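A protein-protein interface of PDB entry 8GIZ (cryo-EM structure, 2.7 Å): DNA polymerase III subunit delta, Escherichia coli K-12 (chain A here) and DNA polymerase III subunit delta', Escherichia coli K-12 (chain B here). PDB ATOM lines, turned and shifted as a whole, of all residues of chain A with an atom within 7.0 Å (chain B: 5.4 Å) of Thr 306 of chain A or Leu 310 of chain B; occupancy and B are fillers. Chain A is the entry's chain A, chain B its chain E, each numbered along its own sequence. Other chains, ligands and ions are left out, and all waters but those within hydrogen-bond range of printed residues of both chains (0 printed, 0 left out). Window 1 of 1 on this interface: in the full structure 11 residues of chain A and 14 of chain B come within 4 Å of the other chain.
Among the printed residues, merely in contact across the chains: Glu 309 of chain A with Leu 310 of chain B (3.3 Å), Thr 306 of chain A with Leu 310 of chain B (3.4 Å), Gln 251 of chain A with Leu 310 of chain B (3.5 Å), Val 302 of chain A with Leu 310 of chain B (3.7 Å), Leu 255 of chain A with Thr 313 of chain B (3.7 Å), Gln 303 of chain A with Asp 314 of chain B (3.7 Å), Glu 309 of chain A with Asn 307 of chain B (3.9 Å) and Val 302 of chain A with Asp 314 of chain B (3.97 Å).
Leu 310 of chain B touches just these residues of chain A: Gln 251 (3.5 Å), Val 302 (3.7 Å), Thr 306 (3.4 Å) and Glu 309 (3.3 Å).
Of the printed residues of chain A, Asp 314 of chain B touches Val 302, Gln 303 and Thr 306.
Of the printed residues of chain B, Gln 251 of chain A touches Asn 307 (2.6 Å) and Leu 310 (3.5 Å).
Printed residues of chain B within 4 Å of Gln 303 of chain A: Asp 314 (3.7 Å).
Leu 305 of chain A touches none of the printed residues of chain B.
The nearest residue of chain B that does not touch Thr 306 of chain A is Leu 311 of chain B (4.7 Å).
The nearest printed residue of chain B that does not touch Val 302 of chain A is Thr 313 of chain B (4.1 Å).
OE1 of Gln 251 of chain A lies within hydrogen-bond range of ND2 of Asn 307 of chain B, 2.6 Å away.
The side-chain hydroxyl (OG1) of Thr 306 of chain A is in hydrogen-bond range of the side-chain carboxylate (OD2) of Asp 314 of chain B.
Of the 9 printed residues of chain B, 4 touch a printed residue of chain A.
Printed residues of chain B that touch a printed residue of chain A: Asn 307, Leu 310, Thr 313 and Asp 314.
Of the 17 printed residues of chain A, 6 touch a printed residue of chain B.
Hydrophobic or aromatic side chains of chain A that line the printed part of chain B: Leu 255 and Val 302.
Among the printed residues, no Asp or Glu carboxylate lies within 4 Å of a Lys or Arg side-chain nitrogen of the other chain.
OE1 of Gln 303 of chain A lies close to O of Gly 343 of chain A (2.9 Å).
The backbone carbonyl oxygen (O) of Gln 303 of chain A is in hydrogen-bond range of the side-chain hydroxyl (OG1) of Thr 306 of chain A (2.6 Å).
OE2 of Glu 309 of chain A is in hydrogen-bond range of NE2 of Gln 251 of chain A (3.0 Å).
The side-chain carboxylate of Glu 309 of chain B sits close to the side-chain amide oxygen of Asn 307 of chain B (3.0 Å).
N of Leu 310 of chain B lies within hydrogen-bond range of OD1 of Asn 307 of chain B, 3.2 Å away.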
ATOM      1  N   GLN A 251       0.479 -18.070   5.001  1.00  0.00           N
ATOM      2  CA  GLN A 251       0.201 -17.116   6.065  1.00  0.00           C
ATOM      3  C   GLN A 251       1.125 -17.330   7.252  1.00  0.00           C
ATOM      4  O   GLN A 251       1.599 -16.364   7.858  1.00  0.00           O
ATOM      5  CB  GLN A 251      -1.259 -17.243   6.500  1.00  0.00           C
ATOM      6  CG  GLN A 251      -1.689 -16.260   7.578  1.00  0.00           C
ATOM      7  CD  GLN A 251      -3.095 -16.525   8.077  1.00  0.00           C
ATOM      8  OE1 GLN A 251      -3.349 -16.509   9.281  1.00  0.00           O
ATOM      9  NE2 GLN A 251      -4.019 -16.767   7.152  1.00  0.00           N
ATOM     10  N   LEU A 254       4.448 -15.916   6.374  1.00  0.00           N
ATOM     11  CA  LEU A 254       4.345 -14.468   6.219  1.00  0.00           C
ATOM     12  C   LEU A 254       4.305 -13.775   7.572  1.00  0.00           C
ATOM     13  O   LEU A 254       4.984 -12.763   7.781  1.00  0.00           O
ATOM     14  CB  LEU A 254       3.103 -14.110   5.403  1.00  0.00           C
ATOM     15  CG  LEU A 254       3.328 -13.727   3.939  1.00  0.00           C
ATOM     16  CD1 LEU A 254       1.997 -13.524   3.238  1.00  0.00           C
ATOM     17  CD2 LEU A 254       4.182 -12.472   3.831  1.00  0.00           C
ATOM     18  N   LEU A 255       3.512 -14.303   8.505  1.00  0.00           N
ATOM     19  CA  LEU A 255       3.456 -13.720   9.839  1.00  0.00           C
ATOM     20  C   LEU A 255       4.798 -13.845  10.545  1.00  0.00           C
ATOM     21  O   LEU A 255       5.241 -12.908  11.223  1.00  0.00           O
ATOM     22  CB  LEU A 255       2.353 -14.388  10.661  1.00  0.00           C
ATOM     23  CG  LEU A 255       0.927 -14.238  10.126  1.00  0.00           C
ATOM     24  CD1 LEU A 255      -0.053 -15.005  11.002  1.00  0.00           C
ATOM     25  CD2 LEU A 255       0.524 -12.779  10.028  1.00  0.00           C
ATOM     26  N   GLN A 300       1.759  -4.989   1.680  1.00  0.00           N
ATOM     27  CA  GLN A 300       0.821  -5.306   0.613  1.00  0.00           C
ATOM     28  C   GLN A 300       0.622  -6.807   0.465  1.00  0.00           C
ATOM     29  O   GLN A 300      -0.424  -7.232  -0.031  1.00  0.00           O
ATOM     30  CB  GLN A 300       1.294  -4.711  -0.717  1.00  0.00           C
ATOM     31  CG  GLN A 300       2.731  -5.040  -1.095  1.00  0.00           C
ATOM     32  CD  GLN A 300       3.709  -3.956  -0.686  1.00  0.00           C
ATOM     33  OE1 GLN A 300       3.409  -3.123   0.168  1.00  0.00           O
ATOM     34  NE2 GLN A 300       4.885  -3.957  -1.301  1.00  0.00           N
ATOM     35  N   ALA A 301       1.598  -7.617   0.884  1.00  0.00           N
ATOM     36  CA  ALA A 301       1.426  -9.065   0.834  1.00  0.00           C
ATOM     37  C   ALA A 301       0.335  -9.526   1.793  1.00  0.00           C
ATOM     38  O   ALA A 301      -0.511 -10.351   1.429  1.00  0.00           O
ATOM     39  CB  ALA A 301       2.747  -9.759   1.154  1.00  0.00           C
ATOM     40  N   VAL A 302       0.333  -9.006   3.022  1.00  0.00           N
ATOM     41  CA  VAL A 302      -0.681  -9.402   3.995  1.00  0.00           C
ATOM     42  C   VAL A 302      -2.061  -8.934   3.550  1.00  0.00           C
ATOM     43  O   VAL A 302      -3.049  -9.673   3.655  1.00  0.00           O
ATOM     44  CB  VAL A 302      -0.321  -8.858   5.388  1.00  0.00           C
ATOM     45  CG1 VAL A 302      -1.388  -9.240   6.401  1.00  0.00           C
ATOM     46  CG2 VAL A 302       1.042  -9.375   5.825  1.00  0.00           C
ATOM     47  N   GLN A 303      -2.157  -7.695   3.061  1.00  0.00           N
ATOM     48  CA  GLN A 303      -3.438  -7.194   2.577  1.00  0.00           C
ATOM     49  C   GLN A 303      -3.924  -8.008   1.387  1.00  0.00           C
ATOM     50  O   GLN A 303      -5.118  -8.307   1.269  1.00  0.00           O
ATOM     51  CB  GLN A 303      -3.312  -5.716   2.208  1.00  0.00           C
ATOM     52  CG  GLN A 303      -4.634  -4.973   2.164  1.00  0.00           C
ATOM     53  CD  GLN A 303      -4.460  -3.496   1.870  1.00  0.00           C
ATOM     54  OE1 GLN A 303      -3.348  -3.030   1.618  1.00  0.00           O
ATOM     55  NE2 GLN A 303      -5.559  -2.752   1.903  1.00  0.00           N
ATOM     56  N   LEU A 304      -3.005  -8.382   0.495  1.00  0.00           N
ATOM     57  CA  LEU A 304      -3.363  -9.227  -0.636  1.00  0.00           C
ATOM     58  C   LEU A 304      -3.867 -10.585  -0.168  1.00  0.00           C
ATOM     59  O   LEU A 304      -4.838 -11.118  -0.713  1.00  0.00           O
ATOM     60  CB  LEU A 304      -2.152  -9.384  -1.555  1.00  0.00           C
ATOM     61  CG  LEU A 304      -2.223 -10.441  -2.653  1.00  0.00           C
ATOM     62  CD1 LEU A 304      -3.502 -10.308  -3.452  1.00  0.00           C
ATOM     63  CD2 LEU A 304      -1.008 -10.310  -3.555  1.00  0.00           C
ATOM     64  N   LEU A 305      -3.217 -11.164   0.842  1.00  0.00           N
ATOM     65  CA  LEU A 305      -3.663 -12.452   1.363  1.00  0.00           C
ATOM     66  C   LEU A 305      -5.059 -12.346   1.967  1.00  0.00           C
ATOM     67  O   LEU A 305      -5.904 -13.228   1.766  1.00  0.00           O
ATOM     68  CB  LEU A 305      -2.662 -12.962   2.399  1.00  0.00           C
ATOM     69  CG  LEU A 305      -2.740 -14.442   2.771  1.00  0.00           C
ATOM     70  CD1 LEU A 305      -2.377 -15.324   1.586  1.00  0.00           C
ATOM     71  CD2 LEU A 305      -1.829 -14.728   3.952  1.00  0.00           C
ATOM     72  N   THR A 306      -5.317 -11.271   2.718  1.00  0.00           N
ATOM     73  CA  THR A 306      -6.646 -11.081   3.294  1.00  0.00           C
ATOM     74  C   THR A 306      -7.694 -10.919   2.200  1.00  0.00           C
ATOM     75  O   THR A 306      -8.788 -11.493   2.284  1.00  0.00           O
ATOM     76  CB  THR A 306      -6.657  -9.865   4.220  1.00  0.00           C
ATOM     77  OG1 THR A 306      -6.418  -8.677   3.457  1.00  0.00           O
ATOM     78  CG2 THR A 306      -5.592  -9.991   5.300  1.00  0.00           C
ATOM     79  N   ARG A 307      -7.376 -10.139   1.165  1.00  0.00           N
ATOM     80  CA  ARG A 307      -8.297  -9.987   0.044  1.00  0.00           C
ATOM     81  C   ARG A 307      -8.553 -11.327  -0.633  1.00  0.00           C
ATOM     82  O   ARG A 307      -9.683 -11.623  -1.035  1.00  0.00           O
ATOM     83  CB  ARG A 307      -7.735  -8.979  -0.959  1.00  0.00           C
ATOM     84  CG  ARG A 307      -8.612  -8.751  -2.183  1.00  0.00           C
ATOM     85  CD  ARG A 307      -7.956  -7.789  -3.160  1.00  0.00           C
ATOM     86  NE  ARG A 307      -7.656  -8.427  -4.437  1.00  0.00           N
ATOM     87  CZ  ARG A 307      -8.529  -8.587  -5.422  1.00  0.00           C
ATOM     88  NH1 ARG A 307      -9.784  -8.181  -5.312  1.00  0.00           N
ATOM     89  NH2 ARG A 307      -8.133  -9.172  -6.550  1.00  0.00           N
ATOM     90  N   THR A 308      -7.506 -12.139  -0.785  1.00  0.00           N
ATOM     91  CA  THR A 308      -7.665 -13.453  -1.395  1.00  0.00           C
ATOM     92  C   THR A 308      -8.611 -14.318  -0.576  1.00  0.00           C
ATOM     93  O   THR A 308      -9.513 -14.961  -1.121  1.00  0.00           O
ATOM     94  CB  THR A 308      -6.303 -14.135  -1.531  1.00  0.00           C
ATOM     95  OG1 THR A 308      -5.370 -13.236  -2.144  1.00  0.00           O
ATOM     96  CG2 THR A 308      -6.417 -15.396  -2.374  1.00  0.00           C
ATOM     97  N   GLU A 309      -8.424 -14.337   0.745  1.00  0.00           N
ATOM     98  CA  GLU A 309      -9.301 -15.136   1.596  1.00  0.00           C
ATOM     99  C   GLU A 309     -10.743 -14.654   1.507  1.00  0.00           C
ATOM    100  O   GLU A 309     -11.677 -15.465   1.435  1.00  0.00           O
ATOM    101  CB  GLU A 309      -8.813 -15.094   3.044  1.00  0.00           C
ATOM    102  CG  GLU A 309      -7.499 -15.817   3.273  1.00  0.00           C
ATOM    103  CD  GLU A 309      -7.169 -15.968   4.744  1.00  0.00           C
ATOM    104  OE1 GLU A 309      -7.958 -15.485   5.582  1.00  0.00           O
ATOM    105  OE2 GLU A 309      -6.124 -16.575   5.062  1.00  0.00           O
ATOM    106  N   LEU A 310     -10.945 -13.335   1.527  1.00  0.00           N
ATOM    107  CA  LEU A 310     -12.299 -12.798   1.436  1.00  0.00           C
ATOM    108  C   LEU A 310     -12.951 -13.180   0.113  1.00  0.00           C
ATOM    109  O   LEU A 310     -14.071 -13.700   0.088  1.00  0.00           O
ATOM    110  CB  LEU A 310     -12.275 -11.279   1.610  1.00  0.00           C
ATOM    111  CG  LEU A 310     -12.560 -10.765   3.024  1.00  0.00           C
ATOM    112  CD1 LEU A 310     -11.612 -11.379   4.044  1.00  0.00           C
ATOM    113  CD2 LEU A 310     -12.473  -9.247   3.061  1.00  0.00           C
ATOM    114  N   THR A 311     -12.259 -12.941  -1.002  1.00  0.00           N
ATOM    115  CA  THR A 311     -12.812 -13.297  -2.303  1.00  0.00           C
ATOM    116  C   THR A 311     -12.990 -14.801  -2.453  1.00  0.00           C
ATOM    117  O   THR A 311     -13.791 -15.240  -3.287  1.00  0.00           O
ATOM    118  CB  THR A 311     -11.913 -12.772  -3.425  1.00  0.00           C
ATOM    119  OG1 THR A 311     -10.586 -13.286  -3.262  1.00  0.00           O
ATOM    120  CG2 THR A 311     -11.873 -11.249  -3.412  1.00  0.00           C
ATOM    121  N   LEU A 312     -12.262 -15.599  -1.671  1.00  0.00           N
ATOM    122  CA  LEU A 312     -12.408 -17.048  -1.732  1.00  0.00           C
ATOM    123  C   LEU A 312     -13.674 -17.505  -1.021  1.00  0.00           C
ATOM    124  O   LEU A 312     -14.534 -18.160  -1.621  1.00  0.00           O
ATOM    125  CB  LEU A 312     -11.173 -17.717  -1.119  1.00  0.00           C
ATOM    126  CG  LEU A 312     -11.283 -19.188  -0.701  1.00  0.00           C
ATOM    127  CD1 LEU A 312     -11.682 -20.081  -1.868  1.00  0.00           C
ATOM    128  CD2 LEU A 312      -9.969 -19.654  -0.100  1.00  0.00           C
ATOM    129  N   GLY A 343      -4.049  -4.958  -3.856  1.00  0.00           N
ATOM    130  CA  GLY A 343      -3.446  -5.230  -2.566  1.00  0.00           C
ATOM    131  C   GLY A 343      -3.905  -4.255  -1.500  1.00  0.00           C
ATOM    132  O   GLY A 343      -3.285  -3.214  -1.280  1.00  0.00           O
ATOM    133  OXT GLY A 343      -4.912  -4.483  -0.833  1.00  0.00           O
ATOM    134  N   ASN B 307      -9.862 -16.049   9.522  1.00  0.00           N
ATOM    135  CA  ASN B 307      -8.613 -16.120  10.270  1.00  0.00           C
ATOM    136  C   ASN B 307      -8.463 -14.854  11.105  1.00  0.00           C
ATOM    137  O   ASN B 307      -8.179 -13.777  10.572  1.00  0.00           O
ATOM    138  CB  ASN B 307      -7.435 -16.300   9.320  1.00  0.00           C
ATOM    139  CG  ASN B 307      -6.180 -16.748  10.035  1.00  0.00           C
ATOM    140  OD1 ASN B 307      -5.787 -16.164  11.043  1.00  0.00           O
ATOM    141  ND2 ASN B 307      -5.552 -17.801   9.527  1.00  0.00           N
ATOM    142  N   ARG B 308      -8.655 -14.987  12.417  1.00  0.00           N
ATOM    143  CA  ARG B 308      -8.697 -13.823  13.294  1.00  0.00           C
ATOM    144  C   ARG B 308      -7.371 -13.070  13.281  1.00  0.00           C
ATOM    145  O   ARG B 308      -7.335 -11.853  13.055  1.00  0.00           O
ATOM    146  CB  ARG B 308      -9.048 -14.275  14.711  1.00  0.00           C
ATOM    147  CG  ARG B 308      -9.254 -13.158  15.717  1.00  0.00           C
ATOM    148  CD  ARG B 308      -8.752 -13.587  17.082  1.00  0.00           C
ATOM    149  NE  ARG B 308      -9.307 -14.876  17.480  1.00  0.00           N
ATOM    150  CZ  ARG B 308      -8.796 -15.660  18.421  1.00  0.00           C
ATOM    151  NH1 ARG B 308      -7.701 -15.324  19.084  1.00  0.00           N
ATOM    152  NH2 ARG B 308      -9.398 -16.811  18.701  1.00  0.00           N
ATOM    153  N   GLU B 309      -6.266 -13.779  13.522  1.00  0.00           N
ATOM    154  CA  GLU B 309      -4.974 -13.107  13.626  1.00  0.00           C
ATOM    155  C   GLU B 309      -4.591 -12.444  12.310  1.00  0.00           C
ATOM    156  O   GLU B 309      -3.994 -11.363  12.305  1.00  0.00           O
ATOM    157  CB  GLU B 309      -3.890 -14.093  14.073  1.00  0.00           C
ATOM    158  CG  GLU B 309      -3.728 -15.343  13.210  1.00  0.00           C
ATOM    159  CD  GLU B 309      -4.595 -16.503  13.670  1.00  0.00           C
ATOM    160  OE1 GLU B 309      -5.497 -16.285  14.506  1.00  0.00           O
ATOM    161  OE2 GLU B 309      -4.371 -17.636  13.195  1.00  0.00           O
ATOM    162  N   LEU B 310      -4.931 -13.073  11.184  1.00  0.00           N
ATOM    163  CA  LEU B 310      -4.613 -12.488   9.885  1.00  0.00           C
ATOM    164  C   LEU B 310      -5.312 -11.146   9.708  1.00  0.00           C
ATOM    165  O   LEU B 310      -4.687 -10.148   9.327  1.00  0.00           O
ATOM    166  CB  LEU B 310      -5.010 -13.462   8.773  1.00  0.00           C
ATOM    167  CG  LEU B 310      -4.479 -13.291   7.342  1.00  0.00           C
ATOM    168  CD1 LEU B 310      -5.652 -13.226   6.376  1.00  0.00           C
ATOM    169  CD2 LEU B 310      -3.565 -12.084   7.153  1.00  0.00           C
ATOM    170  N   LEU B 311      -6.616 -11.097   9.991  1.00  0.00           N
ATOM    171  CA  LEU B 311      -7.348  -9.843   9.857  1.00  0.00           C
ATOM    172  C   LEU B 311      -6.831  -8.797  10.834  1.00  0.00           C
ATOM    173  O   LEU B 311      -6.696  -7.620  10.480  1.00  0.00           O
ATOM    174  CB  LEU B 311      -8.843 -10.080  10.066  1.00  0.00           C
ATOM    175  CG  LEU B 311      -9.655 -10.433   8.818  1.00  0.00           C
ATOM    176  CD1 LEU B 311      -9.768  -9.235   7.887  1.00  0.00           C
ATOM    177  CD2 LEU B 311      -9.046 -11.618   8.086  1.00  0.00           C
ATOM    178  N   ILE B 312      -6.533  -9.201  12.071  1.00  0.00           N
ATOM    179  CA  ILE B 312      -6.071  -8.232  13.063  1.00  0.00           C
ATOM    180  C   ILE B 312      -4.731  -7.636  12.641  1.00  0.00           C
ATOM    181  O   ILE B 312      -4.525  -6.419  12.715  1.00  0.00           O
ATOM    182  CB  ILE B 312      -5.994  -8.879  14.458  1.00  0.00           C
ATOM    183  CG1 ILE B 312      -7.399  -9.259  14.933  1.00  0.00           C
ATOM    184  CG2 ILE B 312      -5.342  -7.916  15.452  1.00  0.00           C
ATOM    185  CD1 ILE B 312      -7.432 -10.084  16.205  1.00  0.00           C
ATOM    186  N   THR B 313      -3.798  -8.480  12.194  1.00  0.00           N
ATOM    187  CA  THR B 313      -2.494  -7.958  11.796  1.00  0.00           C
ATOM    188  C   THR B 313      -2.593  -7.132  10.519  1.00  0.00           C
ATOM    189  O   THR B 313      -1.861  -6.148  10.367  1.00  0.00           O
ATOM    190  CB  THR B 313      -1.482  -9.094  11.625  1.00  0.00           C
ATOM    191  OG1 THR B 313      -0.178  -8.543  11.404  1.00  0.00           O
ATOM    192  CG2 THR B 313      -1.845  -9.990  10.456  1.00  0.00           C
ATOM    193  N   ASP B 314      -3.487  -7.500   9.598  1.00  0.00           N
ATOM    194  CA  ASP B 314      -3.714  -6.656   8.430  1.00  0.00           C
ATOM    195  C   ASP B 314      -4.228  -5.285   8.848  1.00  0.00           C
ATOM    196  O   ASP B 314      -3.791  -4.258   8.315  1.00  0.00           O
ATOM    197  CB  ASP B 314      -4.698  -7.335   7.479  1.00  0.00           C
ATOM    198  CG  ASP B 314      -4.898  -6.558   6.194  1.00  0.00           C
ATOM    199  OD1 ASP B 314      -4.154  -5.583   5.962  1.00  0.00           O
ATOM    200  OD2 ASP B 314      -5.804  -6.922   5.414  1.00  0.00           O
ATOM    201  N   LEU B 315      -5.157  -5.252   9.805  1.00  0.00           N
ATOM    202  CA  LEU B 315      -5.650  -3.977  10.313  1.00  0.00           C
ATOM    203  C   LEU B 315      -4.527  -3.166  10.942  1.00  0.00           C
ATOM    204  O   LEU B 315      -4.430  -1.954  10.725  1.00  0.00           O
ATOM    205  CB  LEU B 315      -6.771  -4.220  11.325  1.00  0.00           C
ATOM    206  CG  LEU B 315      -7.235  -3.025  12.165  1.00  0.00           C
ATOM    207  CD1 LEU B 315      -8.736  -3.079  12.379  1.00  0.00           C
ATOM    208  CD2 LEU B 315      -6.518  -2.980  13.510  1.00  0.00           C
